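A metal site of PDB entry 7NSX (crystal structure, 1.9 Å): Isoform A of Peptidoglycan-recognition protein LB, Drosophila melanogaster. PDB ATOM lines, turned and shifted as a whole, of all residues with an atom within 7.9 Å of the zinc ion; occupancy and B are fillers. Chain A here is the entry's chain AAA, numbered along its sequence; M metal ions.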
ATOM      1  N   ILE A  42      -8.330  26.459 -22.741  1.00  0.00           N
ATOM      2  CA  ILE A  42      -9.345  26.243 -23.802  1.00  0.00           C
ATOM      3  C   ILE A  42     -10.489  27.233 -23.621  1.00  0.00           C
ATOM      4  O   ILE A  42     -11.095  27.242 -22.528  1.00  0.00           O
ATOM      5  CB  ILE A  42      -9.814  24.784 -23.844  1.00  0.00           C
ATOM      6  CG1 ILE A  42      -8.625  23.863 -24.171  1.00  0.00           C
ATOM      7  CG2 ILE A  42     -10.952  24.640 -24.851  1.00  0.00           C
ATOM      8  CD1 ILE A  42      -8.845  22.484 -23.724  1.00  0.00           C
ATOM      9  N   ILE A  43     -10.796  27.985 -24.679  1.00  0.00           N
ATOM     10  CA  ILE A  43     -11.849  29.037 -24.682  1.00  0.00           C
ATOM     11  C   ILE A  43     -13.125  28.430 -25.249  1.00  0.00           C
ATOM     12  O   ILE A  43     -13.081  27.724 -26.319  1.00  0.00           O
ATOM     13  CB  ILE A  43     -11.378  30.282 -25.455  1.00  0.00           C
ATOM     14  CG1 ILE A  43     -10.043  30.805 -24.923  1.00  0.00           C
ATOM     15  CG2 ILE A  43     -12.461  31.367 -25.394  1.00  0.00           C
ATOM     16  CD1 ILE A  43     -10.057  31.221 -23.470  1.00  0.00           C
ATOM     17  N   HIS A  44     -14.216  28.698 -24.537  1.00  0.00           N
ATOM     18  CA  HIS A  44     -15.617  28.363 -24.874  1.00  0.00           C
ATOM     19  C   HIS A  44     -16.453  29.642 -24.888  1.00  0.00           C
ATOM     20  O   HIS A  44     -16.097  30.662 -24.217  1.00  0.00           O
ATOM     21  CB  HIS A  44     -16.196  27.402 -23.814  1.00  0.00           C
ATOM     22  CG  HIS A  44     -15.405  26.152 -23.593  1.00  0.00           C
ATOM     23  ND1 HIS A  44     -15.669  24.975 -24.263  1.00  0.00           N
ATOM     24  CD2 HIS A  44     -14.375  25.884 -22.757  1.00  0.00           C
ATOM     25  CE1 HIS A  44     -14.835  24.050 -23.878  1.00  0.00           C
ATOM     26  NE2 HIS A  44     -14.033  24.574 -22.951  1.00  0.00           N
ATOM     27  N   HIS A  45     -17.639  29.566 -25.491  1.00  0.00           N
ATOM     28  CA  HIS A  45     -18.781  30.468 -25.159  1.00  0.00           C
ATOM     29  C   HIS A  45     -19.896  29.592 -24.578  1.00  0.00           C
ATOM     30  O   HIS A  45     -19.883  28.369 -24.800  1.00  0.00           O
ATOM     31  CB  HIS A  45     -19.176  31.338 -26.372  1.00  0.00           C
ATOM     32  CG  HIS A  45     -19.875  30.610 -27.475  1.00  0.00           C
ATOM     33  ND1 HIS A  45     -20.623  31.287 -28.430  1.00  0.00           N
ATOM     34  CD2 HIS A  45     -19.988  29.279 -27.751  1.00  0.00           C
ATOM     35  CE1 HIS A  45     -21.181  30.387 -29.250  1.00  0.00           C
ATOM     36  NE2 HIS A  45     -20.764  29.149 -28.876  1.00  0.00           N
ATOM     37  N   SER A  46     -20.768  30.194 -23.782  1.00  0.00           N
ATOM     38  CA  SER A  46     -21.900  29.473 -23.134  1.00  0.00           C
ATOM     39  C   SER A  46     -22.950  29.170 -24.212  1.00  0.00           C
ATOM     40  O   SER A  46     -23.554  28.075 -24.131  1.00  0.00           O
ATOM     41  CB  SER A  46     -22.473  30.202 -21.961  1.00  0.00           C
ATOM     42  OG  SER A  46     -22.998  31.462 -22.323  1.00  0.00           O
ATOM     43  N   TYR A  80     -16.891  24.028 -16.555  1.00  0.00           N
ATOM     44  CA  TYR A  80     -15.799  24.972 -16.875  1.00  0.00           C
ATOM     45  C   TYR A  80     -14.972  25.270 -15.630  1.00  0.00           C
ATOM     46  O   TYR A  80     -15.482  25.197 -14.469  1.00  0.00           O
ATOM     47  CB  TYR A  80     -16.430  26.252 -17.445  1.00  0.00           C
ATOM     48  CG  TYR A  80     -17.330  26.057 -18.626  1.00  0.00           C
ATOM     49  CD1 TYR A  80     -18.708  26.235 -18.513  1.00  0.00           C
ATOM     50  CD2 TYR A  80     -16.827  25.689 -19.858  1.00  0.00           C
ATOM     51  CE1 TYR A  80     -19.543  26.115 -19.615  1.00  0.00           C
ATOM     52  CE2 TYR A  80     -17.653  25.566 -20.974  1.00  0.00           C
ATOM     53  CZ  TYR A  80     -19.027  25.758 -20.847  1.00  0.00           C
ATOM     54  OH  TYR A  80     -19.834  25.624 -21.943  1.00  0.00           O
ATOM     55  N   HIS A 102     -15.393  20.034 -19.864  1.00  0.00           N
ATOM     56  CA  HIS A 102     -15.609  21.015 -20.969  1.00  0.00           C
ATOM     57  C   HIS A 102     -14.945  20.563 -22.270  1.00  0.00           C
ATOM     58  O   HIS A 102     -15.363  21.096 -23.315  1.00  0.00           O
ATOM     59  CB  HIS A 102     -15.134  22.395 -20.536  1.00  0.00           C
ATOM     60  CG  HIS A 102     -13.681  22.430 -20.213  1.00  0.00           C
ATOM     61  ND1 HIS A 102     -12.739  22.725 -21.184  1.00  0.00           N
ATOM     62  CD2 HIS A 102     -13.005  22.185 -19.063  1.00  0.00           C
ATOM     63  CE1 HIS A 102     -11.543  22.619 -20.646  1.00  0.00           C
ATOM     64  NE2 HIS A 102     -11.684  22.316 -19.332  1.00  0.00           N
ATOM     65  N   ALA A 103     -13.924  19.696 -22.243  1.00  0.00           N
ATOM     66  CA  ALA A 103     -13.084  19.422 -23.445  1.00  0.00           C
ATOM     67  C   ALA A 103     -12.478  18.041 -23.310  1.00  0.00           C
ATOM     68  O   ALA A 103     -11.390  17.877 -22.764  1.00  0.00           O
ATOM     69  CB  ALA A 103     -12.017  20.476 -23.604  1.00  0.00           C
ATOM     70  N   ILE A 113     -12.169  28.047 -19.936  1.00  0.00           N
ATOM     71  CA  ILE A 113     -12.728  29.384 -19.627  1.00  0.00           C
ATOM     72  C   ILE A 113     -13.952  29.634 -20.529  1.00  0.00           C
ATOM     73  O   ILE A 113     -13.794  29.521 -21.738  1.00  0.00           O
ATOM     74  CB  ILE A 113     -11.699  30.497 -19.850  1.00  0.00           C
ATOM     75  CG1 ILE A 113     -10.394  30.225 -19.099  1.00  0.00           C
ATOM     76  CG2 ILE A 113     -12.315  31.845 -19.488  1.00  0.00           C
ATOM     77  CD1 ILE A 113      -9.335  31.269 -19.378  1.00  0.00           C
ATOM     78  N   VAL A 114     -15.103  29.927 -19.957  1.00  0.00           N
ATOM     79  CA  VAL A 114     -16.335  30.170 -20.746  1.00  0.00           C
ATOM     80  C   VAL A 114     -16.621  31.677 -20.732  1.00  0.00           C
ATOM     81  O   VAL A 114     -16.693  32.244 -19.656  1.00  0.00           O
ATOM     82  CB  VAL A 114     -17.556  29.346 -20.303  1.00  0.00           C
ATOM     83  CG1 VAL A 114     -18.013  29.666 -18.902  1.00  0.00           C
ATOM     84  CG2 VAL A 114     -18.704  29.549 -21.300  1.00  0.00           C
ATOM     85  N   GLY A 153      -9.263  27.214 -28.924  1.00  0.00           N
ATOM     86  CA  GLY A 153     -10.727  27.205 -28.914  1.00  0.00           C
ATOM     87  C   GLY A 153     -11.213  25.784 -28.871  1.00  0.00           C
ATOM     88  O   GLY A 153     -10.471  24.887 -29.360  1.00  0.00           O
ATOM     89  N   HIS A 154     -12.387  25.570 -28.281  1.00  0.00           N
ATOM     90  CA  HIS A 154     -13.003  24.232 -28.135  1.00  0.00           C
ATOM     91  C   HIS A 154     -13.002  23.566 -29.515  1.00  0.00           C
ATOM     92  O   HIS A 154     -12.623  22.370 -29.573  1.00  0.00           O
ATOM     93  CB  HIS A 154     -14.399  24.385 -27.545  1.00  0.00           C
ATOM     94  CG  HIS A 154     -15.071  23.110 -27.179  1.00  0.00           C
ATOM     95  ND1 HIS A 154     -16.325  23.100 -26.598  1.00  0.00           N
ATOM     96  CD2 HIS A 154     -14.690  21.815 -27.297  1.00  0.00           C
ATOM     97  CE1 HIS A 154     -16.685  21.851 -26.376  1.00  0.00           C
ATOM     98  NE2 HIS A 154     -15.695  21.053 -26.796  1.00  0.00           N
ATOM     99  N   ARG A 155     -13.360  24.317 -30.570  1.00  0.00           N
ATOM    100  CA  ARG A 155     -13.534  23.772 -31.946  1.00  0.00           C
ATOM    101  C   ARG A 155     -12.239  23.164 -32.501  1.00  0.00           C
ATOM    102  O   ARG A 155     -12.301  22.565 -33.591  1.00  0.00           O
ATOM    103  CB  ARG A 155     -13.986  24.853 -32.901  1.00  0.00           C
ATOM    104  CG  ARG A 155     -13.017  26.032 -32.996  1.00  0.00           C
ATOM    105  CD  ARG A 155     -13.352  26.895 -34.191  1.00  0.00           C
ATOM    106  NE  ARG A 155     -14.729  27.349 -34.115  1.00  0.00           N
ATOM    107  CZ  ARG A 155     -15.338  28.078 -35.051  1.00  0.00           C
ATOM    108  NH1 ARG A 155     -14.694  28.440 -36.143  1.00  0.00           N
ATOM    109  NH2 ARG A 155     -16.603  28.433 -34.878  1.00  0.00           N
ATOM    110  N   ARG A 158     -12.508  19.349 -30.825  1.00  0.00           N
ATOM    111  CA  ARG A 158     -13.801  18.650 -30.949  1.00  0.00           C
ATOM    112  C   ARG A 158     -14.552  19.342 -32.068  1.00  0.00           C
ATOM    113  O   ARG A 158     -14.329  20.541 -32.267  1.00  0.00           O
ATOM    114  CB  ARG A 158     -14.601  18.713 -29.643  1.00  0.00           C
ATOM    115  CG  ARG A 158     -16.008  18.121 -29.708  1.00  0.00           C
ATOM    116  CD  ARG A 158     -15.940  16.623 -29.528  1.00  0.00           C
ATOM    117  NE  ARG A 158     -14.992  16.397 -28.442  1.00  0.00           N
ATOM    118  CZ  ARG A 158     -14.041  15.467 -28.445  1.00  0.00           C
ATOM    119  NH1 ARG A 158     -13.905  14.628 -29.451  1.00  0.00           N
ATOM    120  NH2 ARG A 158     -13.228  15.399 -27.407  1.00  0.00           N
ATOM    121  N   THR A 160     -17.216  21.311 -33.174  1.00  0.00           N
ATOM    122  CA  THR A 160     -18.183  22.244 -32.575  1.00  0.00           C
ATOM    123  C   THR A 160     -17.920  23.618 -33.194  1.00  0.00           C
ATOM    124  O   THR A 160     -16.790  23.842 -33.662  1.00  0.00           O
ATOM    125  CB  THR A 160     -18.088  22.166 -31.026  1.00  0.00           C
ATOM    126  OG1 THR A 160     -19.055  23.025 -30.439  1.00  0.00           O
ATOM    127  CG2 THR A 160     -16.737  22.597 -30.506  1.00  0.00           C
ATOM    128  N   GLU A 161     -18.898  24.514 -33.117  1.00  0.00           N
ATOM    129  CA  GLU A 161     -18.735  25.960 -33.393  1.00  0.00           C
ATOM    130  C   GLU A 161     -18.151  26.667 -32.170  1.00  0.00           C
ATOM    131  O   GLU A 161     -17.508  27.694 -32.371  1.00  0.00           O
ATOM    132  CB  GLU A 161     -20.035  26.595 -33.873  1.00  0.00           C
ATOM    133  CG  GLU A 161     -20.333  26.212 -35.318  1.00  0.00           C
ATOM    134  CD  GLU A 161     -21.734  26.583 -35.770  1.00  0.00           C
ATOM    135  OE1 GLU A 161     -22.239  27.634 -35.298  1.00  0.00           O
ATOM    136  OE2 GLU A 161     -22.321  25.802 -36.572  1.00  0.00           O
ATOM    137  N   CYS A 162     -18.319  26.130 -30.961  1.00  0.00           N
ATOM    138  CA  CYS A 162     -17.765  26.721 -29.712  1.00  0.00           C
ATOM    139  C   CYS A 162     -16.291  27.069 -29.947  1.00  0.00           C
ATOM    140  O   CYS A 162     -15.565  26.185 -30.415  1.00  0.00           O
ATOM    141  CB  CYS A 162     -17.888  25.745 -28.562  1.00  0.00           C
ATOM    142  SG  CYS A 162     -17.374  26.486 -26.997  1.00  0.00           S
ATOM    143  N   PRO A 163     -15.775  28.278 -29.644  1.00  0.00           N
ATOM    144  CA  PRO A 163     -16.473  29.337 -28.893  1.00  0.00           C
ATOM    145  C   PRO A 163     -17.198  30.424 -29.721  1.00  0.00           C
ATOM    146  O   PRO A 163     -17.346  31.527 -29.226  1.00  0.00           O
ATOM    147  CB  PRO A 163     -15.295  30.014 -28.160  1.00  0.00           C
ATOM    148  CG  PRO A 163     -14.162  29.955 -29.193  1.00  0.00           C
ATOM    149  CD  PRO A 163     -14.363  28.628 -29.890  1.00  0.00           C
ATOM    150  N   GLY A 164     -17.653  30.079 -30.934  1.00  0.00           N
ATOM    151  CA  GLY A 164     -18.281  31.041 -31.855  1.00  0.00           C
ATOM    152  C   GLY A 164     -17.237  31.595 -32.804  1.00  0.00           C
ATOM    153  O   GLY A 164     -16.126  31.912 -32.339  1.00  0.00           O
HETATM  154 ZN    ZN M   1     -17.162  24.737 -25.710  1.00  0.00          ZN
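The backbone carbonyl oxygen of His 102 lies close to a ring nitrogen (NE2) of His 154.
The backbone carbonyl oxygen (O) of Ile 43 is in hydrogen-bond range of the backbone NH (N) of His 154, 3.0 Å away.
A ring nitrogen (NE2) of His 44 lies within hydrogen-bond range of a ring nitrogen (ND1) of His 102 (2.9 Å).
The backbone carbonyl oxygen (O) of Ile 113 sits at hydrogen-bond distance from the backbone NH (N) of His 44 (2.9 Å).
The side-chain sulfur (SG) of Cys 162 lies close to the backbone NH (N) of His 45.
The side-chain hydroxyl (OG1) of Thr 160 is in hydrogen-bond range of the backbone NH (N) of Cys 162, at 3.2 Å.
The backbone carbonyl oxygen (O) of Cys 162 is in hydrogen-bond range of the backbone NH (N) of Arg 155, at 2.9 Å.
Within 4 Å of the zinc ion: His 44, His 154 and Cys 162.
Along chain A the residues within 4 Å of the zinc ion span positions 44 to 162.
The nearest printed residue that does not touch the zinc ion is His 45 (4.6 Å).
The zinc ion is bound by ND1 of His 154, ND1 of His 44 and SG of Cys 162.
The zinc ion has three donor atoms within binding distance.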
